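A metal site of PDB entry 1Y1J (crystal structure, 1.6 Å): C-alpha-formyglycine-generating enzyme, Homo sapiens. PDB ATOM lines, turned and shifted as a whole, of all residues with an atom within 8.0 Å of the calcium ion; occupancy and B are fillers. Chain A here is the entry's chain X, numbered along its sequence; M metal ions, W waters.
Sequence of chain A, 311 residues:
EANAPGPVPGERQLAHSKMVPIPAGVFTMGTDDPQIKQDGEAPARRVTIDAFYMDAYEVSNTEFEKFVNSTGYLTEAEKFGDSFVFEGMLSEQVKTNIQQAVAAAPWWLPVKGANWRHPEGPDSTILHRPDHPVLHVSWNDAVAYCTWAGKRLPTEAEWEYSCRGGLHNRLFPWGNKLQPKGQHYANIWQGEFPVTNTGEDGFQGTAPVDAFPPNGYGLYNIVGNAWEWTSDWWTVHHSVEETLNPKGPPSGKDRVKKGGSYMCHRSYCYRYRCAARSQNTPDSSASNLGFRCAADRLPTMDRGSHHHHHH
The side-chain amide oxygen (OD1) of Asn 225 sits at hydrogen-bond distance from the side-chain amide nitrogen (ND2) of Asn 187.
The backbone NH of Ala 207 lies close to the side-chain amide nitrogen of Asn 187 (3.4 Å).
The backbone carbonyl oxygen (O) of Gly 205 sits at hydrogen-bond distance from the side-chain amide nitrogen (ND2) of Asn 187 (2.8 Å).
OE1 of Gln 190 is in hydrogen-bond range of N of Asp 201, 2.9 Å away.
The nearest printed residue that does not touch the calcium ion is Gln 190 (4.1 Å).
OD1 of Asn 187 is bound to the calcium ion (2.3 Å).
The calcium ion is bound by O of Phe 203 (2.3 Å).
The backbone carbonyl oxygen (O) of Ile 188 is bound to the calcium ion, 2.3 Å away.
Water W1 is bound to the calcium ion, 2.4 Å away.
The calcium ion is bound by OD2 of Asp 201.
The calcium ion is bound by water W2, 2.4 Å away.
OD1 of Asp 201 binds the calcium ion (2.5 Å).
The calcium ion has seven donor atoms within binding distance.
Water W1 bridges the side-chain amide oxygen (OD1) of Asn 197 (2.7 Å) and the side-chain amide oxygen (OE1) of Gln 190 (2.7 Å).
Water W2 lies within hydrogen-bond range of O of Tyr 262 (2.7 Å), O of Gln 204 (2.7 Å) and ND2 of Asn 197 (3.0 Å).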
ATOM      1  N   HIS A 184      14.828  -2.590   0.146  1.00  0.00           N
ATOM      2  CA  HIS A 184      14.674  -1.855  -1.126  1.00  0.00           C
ATOM      3  C   HIS A 184      14.677  -2.830  -2.309  1.00  0.00           C
ATOM      4  O   HIS A 184      15.582  -3.682  -2.417  1.00  0.00           O
ATOM      5  CB  HIS A 184      15.747  -0.779  -1.277  1.00  0.00           C
ATOM      6  CG  HIS A 184      15.483   0.445  -0.432  1.00  0.00           C
ATOM      7  ND1 HIS A 184      14.543   1.392  -0.801  1.00  0.00           N
ATOM      8  CD2 HIS A 184      15.993   0.863   0.744  1.00  0.00           C
ATOM      9  CE1 HIS A 184      14.485   2.328   0.125  1.00  0.00           C
ATOM     10  NE2 HIS A 184      15.354   2.032   1.071  1.00  0.00           N
ATOM     11  N   ALA A 186      13.934  -1.601  -5.701  1.00  0.00           N
ATOM     12  CA  ALA A 186      14.152  -0.827  -6.915  1.00  0.00           C
ATOM     13  C   ALA A 186      14.896   0.456  -6.617  1.00  0.00           C
ATOM     14  O   ALA A 186      14.858   0.956  -5.488  1.00  0.00           O
ATOM     15  CB  ALA A 186      12.820  -0.500  -7.613  1.00  0.00           C
ATOM     16  N   ASN A 187      15.533   0.996  -7.647  1.00  0.00           N
ATOM     17  CA  ASN A 187      16.284   2.241  -7.538  1.00  0.00           C
ATOM     18  C   ASN A 187      15.401   3.419  -7.949  1.00  0.00           C
ATOM     19  O   ASN A 187      15.245   3.683  -9.100  1.00  0.00           O
ATOM     20  CB  ASN A 187      17.551   2.202  -8.413  1.00  0.00           C
ATOM     21  CG  ASN A 187      18.368   3.490  -8.303  1.00  0.00           C
ATOM     22  OD1 ASN A 187      18.194   4.232  -7.336  1.00  0.00           O
ATOM     23  ND2 ASN A 187      19.282   3.752  -9.275  1.00  0.00           N
ATOM     24  N   ILE A 188      14.817   4.073  -6.951  1.00  0.00           N
ATOM     25  CA  ILE A 188      14.057   5.308  -7.147  1.00  0.00           C
ATOM     26  C   ILE A 188      14.630   6.398  -6.208  1.00  0.00           C
ATOM     27  O   ILE A 188      15.772   6.291  -5.731  1.00  0.00           O
ATOM     28  CB  ILE A 188      12.560   5.046  -6.979  1.00  0.00           C
ATOM     29  CG1 ILE A 188      12.215   4.524  -5.590  1.00  0.00           C
ATOM     30  CG2 ILE A 188      12.087   4.086  -8.043  1.00  0.00           C
ATOM     31  CD1 ILE A 188      10.705   4.478  -5.338  1.00  0.00           C
ATOM     32  N   TRP A 189      13.855   7.442  -5.952  1.00  0.00           N
ATOM     33  CA  TRP A 189      14.308   8.549  -5.104  1.00  0.00           C
ATOM     34  C   TRP A 189      13.842   8.382  -3.664  1.00  0.00           C
ATOM     35  O   TRP A 189      12.724   7.978  -3.415  1.00  0.00           O
ATOM     36  CB  TRP A 189      13.666   9.816  -5.640  1.00  0.00           C
ATOM     37  CG  TRP A 189      14.129  11.116  -5.068  1.00  0.00           C
ATOM     38  CD1 TRP A 189      13.753  11.693  -3.881  1.00  0.00           C
ATOM     39  CD2 TRP A 189      15.029  12.034  -5.697  1.00  0.00           C
ATOM     40  NE1 TRP A 189      14.388  12.904  -3.733  1.00  0.00           N
ATOM     41  CE2 TRP A 189      15.150  13.157  -4.849  1.00  0.00           C
ATOM     42  CE3 TRP A 189      15.735  12.020  -6.909  1.00  0.00           C
ATOM     43  CZ2 TRP A 189      15.968  14.248  -5.166  1.00  0.00           C
ATOM     44  CZ3 TRP A 189      16.537  13.122  -7.230  1.00  0.00           C
ATOM     45  CH2 TRP A 189      16.626  14.223  -6.362  1.00  0.00           C
ATOM     46  N   GLN A 190      14.727   8.698  -2.715  1.00  0.00           N
ATOM     47  CA  GLN A 190      14.296   8.889  -1.328  1.00  0.00           C
ATOM     48  C   GLN A 190      14.694  10.281  -0.939  1.00  0.00           C
ATOM     49  O   GLN A 190      15.772  10.720  -1.308  1.00  0.00           O
ATOM     50  CB  GLN A 190      14.943   7.895  -0.385  1.00  0.00           C
ATOM     51  CG  GLN A 190      14.533   6.454  -0.617  1.00  0.00           C
ATOM     52  CD  GLN A 190      15.407   5.799  -1.664  1.00  0.00           C
ATOM     53  OE1 GLN A 190      16.628   5.992  -1.652  1.00  0.00           O
ATOM     54  NE2 GLN A 190      14.784   5.001  -2.572  1.00  0.00           N
ATOM     55  N   ASN A 197      18.261  13.987  -2.626  1.00  0.00           N
ATOM     56  CA  ASN A 197      18.171  12.536  -2.767  1.00  0.00           C
ATOM     57  C   ASN A 197      19.098  11.936  -1.738  1.00  0.00           C
ATOM     58  O   ASN A 197      20.310  12.110  -1.813  1.00  0.00           O
ATOM     59  CB  ASN A 197      18.628  12.097  -4.156  1.00  0.00           C
ATOM     60  CG  ASN A 197      18.343  10.628  -4.442  1.00  0.00           C
ATOM     61  OD1 ASN A 197      18.143   9.840  -3.526  1.00  0.00           O
ATOM     62  ND2 ASN A 197      18.317  10.267  -5.706  1.00  0.00           N
ATOM     63  N   THR A 198      18.535  11.199  -0.784  1.00  0.00           N
ATOM     64  CA  THR A 198      19.331  10.718   0.340  1.00  0.00           C
ATOM     65  C   THR A 198      20.191   9.528  -0.068  1.00  0.00           C
ATOM     66  O   THR A 198      21.164   9.206   0.601  1.00  0.00           O
ATOM     67  CB  THR A 198      18.424  10.265   1.499  1.00  0.00           C
ATOM     68  OG1 THR A 198      17.660   9.137   1.088  1.00  0.00           O
ATOM     69  CG2 THR A 198      17.497  11.381   1.932  1.00  0.00           C
ATOM     70  N   GLY A 199      19.870   8.879  -1.202  1.00  0.00           N
ATOM     71  CA  GLY A 199      20.655   7.724  -1.604  1.00  0.00           C
ATOM     72  C   GLY A 199      20.466   6.552  -0.646  1.00  0.00           C
ATOM     73  O   GLY A 199      21.291   5.659  -0.602  1.00  0.00           O
ATOM     74  N   GLU A 200      19.322   6.527   0.045  1.00  0.00           N
ATOM     75  CA  GLU A 200      19.023   5.468   1.029  1.00  0.00           C
ATOM     76  C   GLU A 200      19.074   4.093   0.383  1.00  0.00           C
ATOM     77  O   GLU A 200      19.556   3.135   1.007  1.00  0.00           O
ATOM     78  CB  GLU A 200      17.653   5.725   1.664  1.00  0.00           C
ATOM     79  CG  GLU A 200      17.152   4.648   2.605  1.00  0.00           C
ATOM     80  CD  GLU A 200      15.692   4.793   2.976  1.00  0.00           C
ATOM     81  OE1 GLU A 200      15.164   5.944   2.944  1.00  0.00           O
ATOM     82  OE2 GLU A 200      15.082   3.745   3.320  1.00  0.00           O
ATOM     83  N   ASP A 201      18.586   3.974  -0.867  1.00  0.00           N
ATOM     84  CA  ASP A 201      18.531   2.672  -1.532  1.00  0.00           C
ATOM     85  C   ASP A 201      19.909   2.207  -2.055  1.00  0.00           C
ATOM     86  O   ASP A 201      20.046   1.130  -2.655  1.00  0.00           O
ATOM     87  CB  ASP A 201      17.441   2.632  -2.605  1.00  0.00           C
ATOM     88  CG  ASP A 201      17.692   3.576  -3.761  1.00  0.00           C
ATOM     89  OD1 ASP A 201      18.843   4.011  -3.935  1.00  0.00           O
ATOM     90  OD2 ASP A 201      16.735   3.899  -4.518  1.00  0.00           O
ATOM     91  N   GLY A 202      20.935   3.025  -1.832  1.00  0.00           N
ATOM     92  CA  GLY A 202      22.275   2.685  -2.277  1.00  0.00           C
ATOM     93  C   GLY A 202      22.788   3.400  -3.517  1.00  0.00           C
ATOM     94  O   GLY A 202      23.960   3.277  -3.834  1.00  0.00           O
ATOM     95  N   PHE A 203      21.923   4.138  -4.223  1.00  0.00           N
ATOM     96  CA  PHE A 203      22.289   4.815  -5.473  1.00  0.00           C
ATOM     97  C   PHE A 203      21.534   6.120  -5.628  1.00  0.00           C
ATOM     98  O   PHE A 203      20.302   6.157  -5.523  1.00  0.00           O
ATOM     99  CB  PHE A 203      21.954   3.905  -6.642  1.00  0.00           C
ATOM    100  CG  PHE A 203      22.581   2.567  -6.513  1.00  0.00           C
ATOM    101  CD1 PHE A 203      23.868   2.382  -6.954  1.00  0.00           C
ATOM    102  CD2 PHE A 203      21.894   1.502  -5.930  1.00  0.00           C
ATOM    103  CE1 PHE A 203      24.491   1.135  -6.795  1.00  0.00           C
ATOM    104  CE2 PHE A 203      22.506   0.268  -5.793  1.00  0.00           C
ATOM    105  CZ  PHE A 203      23.792   0.083  -6.234  1.00  0.00           C
ATOM    106  N   GLN A 204      22.279   7.204  -5.841  1.00  0.00           N
ATOM    107  CA  GLN A 204      21.647   8.478  -6.123  1.00  0.00           C
ATOM    108  C   GLN A 204      21.282   8.587  -7.596  1.00  0.00           C
ATOM    109  O   GLN A 204      20.143   8.947  -7.939  1.00  0.00           O
ATOM    110  CB  GLN A 204      22.553   9.620  -5.696  1.00  0.00           C
ATOM    111  CG  GLN A 204      22.628   9.665  -4.196  1.00  0.00           C
ATOM    112  CD  GLN A 204      23.579  10.687  -3.657  1.00  0.00           C
ATOM    113  OE1 GLN A 204      24.728  10.799  -4.108  1.00  0.00           O
ATOM    114  NE2 GLN A 204      23.125  11.410  -2.639  1.00  0.00           N
ATOM    115  N   GLY A 205      22.233   8.286  -8.468  1.00  0.00           N
ATOM    116  CA  GLY A 205      21.986   8.135  -9.889  1.00  0.00           C
ATOM    117  C   GLY A 205      21.616   6.709 -10.223  1.00  0.00           C
ATOM    118  O   GLY A 205      20.949   6.027  -9.445  1.00  0.00           O
ATOM    119  N   THR A 206      22.060   6.217 -11.393  1.00  0.00           N
ATOM    120  CA  THR A 206      21.825   4.821 -11.751  1.00  0.00           C
ATOM    121  C   THR A 206      22.573   3.816 -10.867  1.00  0.00           C
ATOM    122  O   THR A 206      23.541   4.163 -10.132  1.00  0.00           O
ATOM    123  CB  THR A 206      22.224   4.542 -13.229  1.00  0.00           C
ATOM    124  OG1 THR A 206      23.593   4.916 -13.417  1.00  0.00           O
ATOM    125  CG2 THR A 206      21.342   5.362 -14.148  1.00  0.00           C
ATOM    126  N   ALA A 207      22.061   2.581 -10.903  1.00  0.00           N
ATOM    127  CA  ALA A 207      22.713   1.414 -10.312  1.00  0.00           C
ATOM    128  C   ALA A 207      23.142   0.473 -11.413  1.00  0.00           C
ATOM    129  O   ALA A 207      22.624   0.542 -12.525  1.00  0.00           O
ATOM    130  CB  ALA A 207      21.756   0.689  -9.374  1.00  0.00           C
ATOM    131  N   PHE A 212      19.589  -5.103  -7.344  1.00  0.00           N
ATOM    132  CA  PHE A 212      18.247  -5.337  -6.759  1.00  0.00           C
ATOM    133  C   PHE A 212      17.690  -6.711  -7.155  1.00  0.00           C
ATOM    134  O   PHE A 212      18.216  -7.400  -8.026  1.00  0.00           O
ATOM    135  CB  PHE A 212      17.288  -4.173  -7.076  1.00  0.00           C
ATOM    136  CG  PHE A 212      17.714  -2.855  -6.439  1.00  0.00           C
ATOM    137  CD1 PHE A 212      17.549  -2.621  -5.072  1.00  0.00           C
ATOM    138  CD2 PHE A 212      18.373  -1.894  -7.197  1.00  0.00           C
ATOM    139  CE1 PHE A 212      17.977  -1.459  -4.494  1.00  0.00           C
ATOM    140  CE2 PHE A 212      18.811  -0.715  -6.614  1.00  0.00           C
ATOM    141  CZ  PHE A 212      18.598  -0.489  -5.282  1.00  0.00           C
ATOM    142  N   ASN A 225      15.495   2.776 -11.916  1.00  0.00           N
ATOM    143  CA  ASN A 225      16.833   2.842 -12.501  1.00  0.00           C
ATOM    144  C   ASN A 225      16.746   3.714 -13.761  1.00  0.00           C
ATOM    145  O   ASN A 225      16.744   4.922 -13.631  1.00  0.00           O
ATOM    146  CB  ASN A 225      17.459   1.453 -12.711  1.00  0.00           C
ATOM    147  CG  ASN A 225      18.960   1.455 -12.524  1.00  0.00           C
ATOM    148  OD1 ASN A 225      19.473   2.214 -11.702  1.00  0.00           O
ATOM    149  ND2 ASN A 225      19.682   0.588 -13.251  1.00  0.00           N
ATOM    150  N   SER A 261      12.217   5.695 -13.171  1.00  0.00           N
ATOM    151  CA  SER A 261      13.652   5.827 -13.080  1.00  0.00           C
ATOM    152  C   SER A 261      14.111   6.109 -11.652  1.00  0.00           C
ATOM    153  O   SER A 261      13.292   6.240 -10.734  1.00  0.00           O
ATOM    154  CB  SER A 261      14.110   6.958 -13.984  1.00  0.00           C
ATOM    155  OG  SER A 261      13.848   8.242 -13.402  1.00  0.00           O
ATOM    156  N   TYR A 262      15.421   6.253 -11.497  1.00  0.00           N
ATOM    157  CA  TYR A 262      16.022   6.654 -10.206  1.00  0.00           C
ATOM    158  C   TYR A 262      15.532   7.977  -9.636  1.00  0.00           C
ATOM    159  O   TYR A 262      15.813   8.296  -8.457  1.00  0.00           O
ATOM    160  CB  TYR A 262      17.546   6.665 -10.324  1.00  0.00           C
ATOM    161  CG  TYR A 262      18.152   7.780 -11.160  1.00  0.00           C
ATOM    162  CD1 TYR A 262      18.574   7.576 -12.479  1.00  0.00           C
ATOM    163  CD2 TYR A 262      18.373   9.014 -10.586  1.00  0.00           C
ATOM    164  CE1 TYR A 262      19.161   8.606 -13.185  1.00  0.00           C
ATOM    165  CE2 TYR A 262      18.943  10.041 -11.286  1.00  0.00           C
ATOM    166  CZ  TYR A 262      19.336   9.836 -12.580  1.00  0.00           C
ATOM    167  OH  TYR A 262      19.953  10.848 -13.250  1.00  0.00           O
ATOM    168  N   MET A 263      14.782   8.731 -10.446  1.00  0.00           N
ATOM    169  CA  MET A 263      14.293  10.060 -10.073  1.00  0.00           C
ATOM    170  C   MET A 263      12.924  10.013  -9.442  1.00  0.00           C
ATOM    171  O   MET A 263      12.496  10.983  -8.794  1.00  0.00           O
ATOM    172  CB  MET A 263      14.249  10.989 -11.285  1.00  0.00           C
ATOM    173  CG  MET A 263      15.589  11.446 -11.751  1.00  0.00           C
ATOM    174  SD  MET A 263      15.468  12.367 -13.326  1.00  0.00           S
ATOM    175  CE  MET A 263      14.603  13.866 -12.790  1.00  0.00           C
ATOM    176  N   OCS A 264      12.190   8.914  -9.633  1.00  0.00           N
ATOM    177  CA  OCS A 264      10.781   8.889  -9.249  1.00  0.00           C
ATOM    178  CB  OCS A 264      10.099   7.685  -9.793  1.00  0.00           C
ATOM    179  SG  OCS A 264       9.611   7.791 -11.494  1.00  0.00           S
ATOM    180  C   OCS A 264      10.562   8.879  -7.758  1.00  0.00           C
ATOM    181  O   OCS A 264      11.276   8.226  -7.050  1.00  0.00           O
ATOM    182  OD1 OCS A 264       8.806   6.646 -11.668  1.00  0.00           O
ATOM    183  OD2 OCS A 264       8.788   8.936 -11.748  1.00  0.00           O
ATOM    184  OD3 OCS A 264      10.755   7.837 -12.308  1.00  0.00           O
HETATM  185 CA    CA M   1      18.017   5.682  -5.540  1.00  0.00          CA
HETATM  186  O   HOH W   1      18.005   7.168  -3.634  1.00  0.00           O
HETATM  187  O   HOH W   2      17.962   7.611  -7.032  1.00  0.00           O
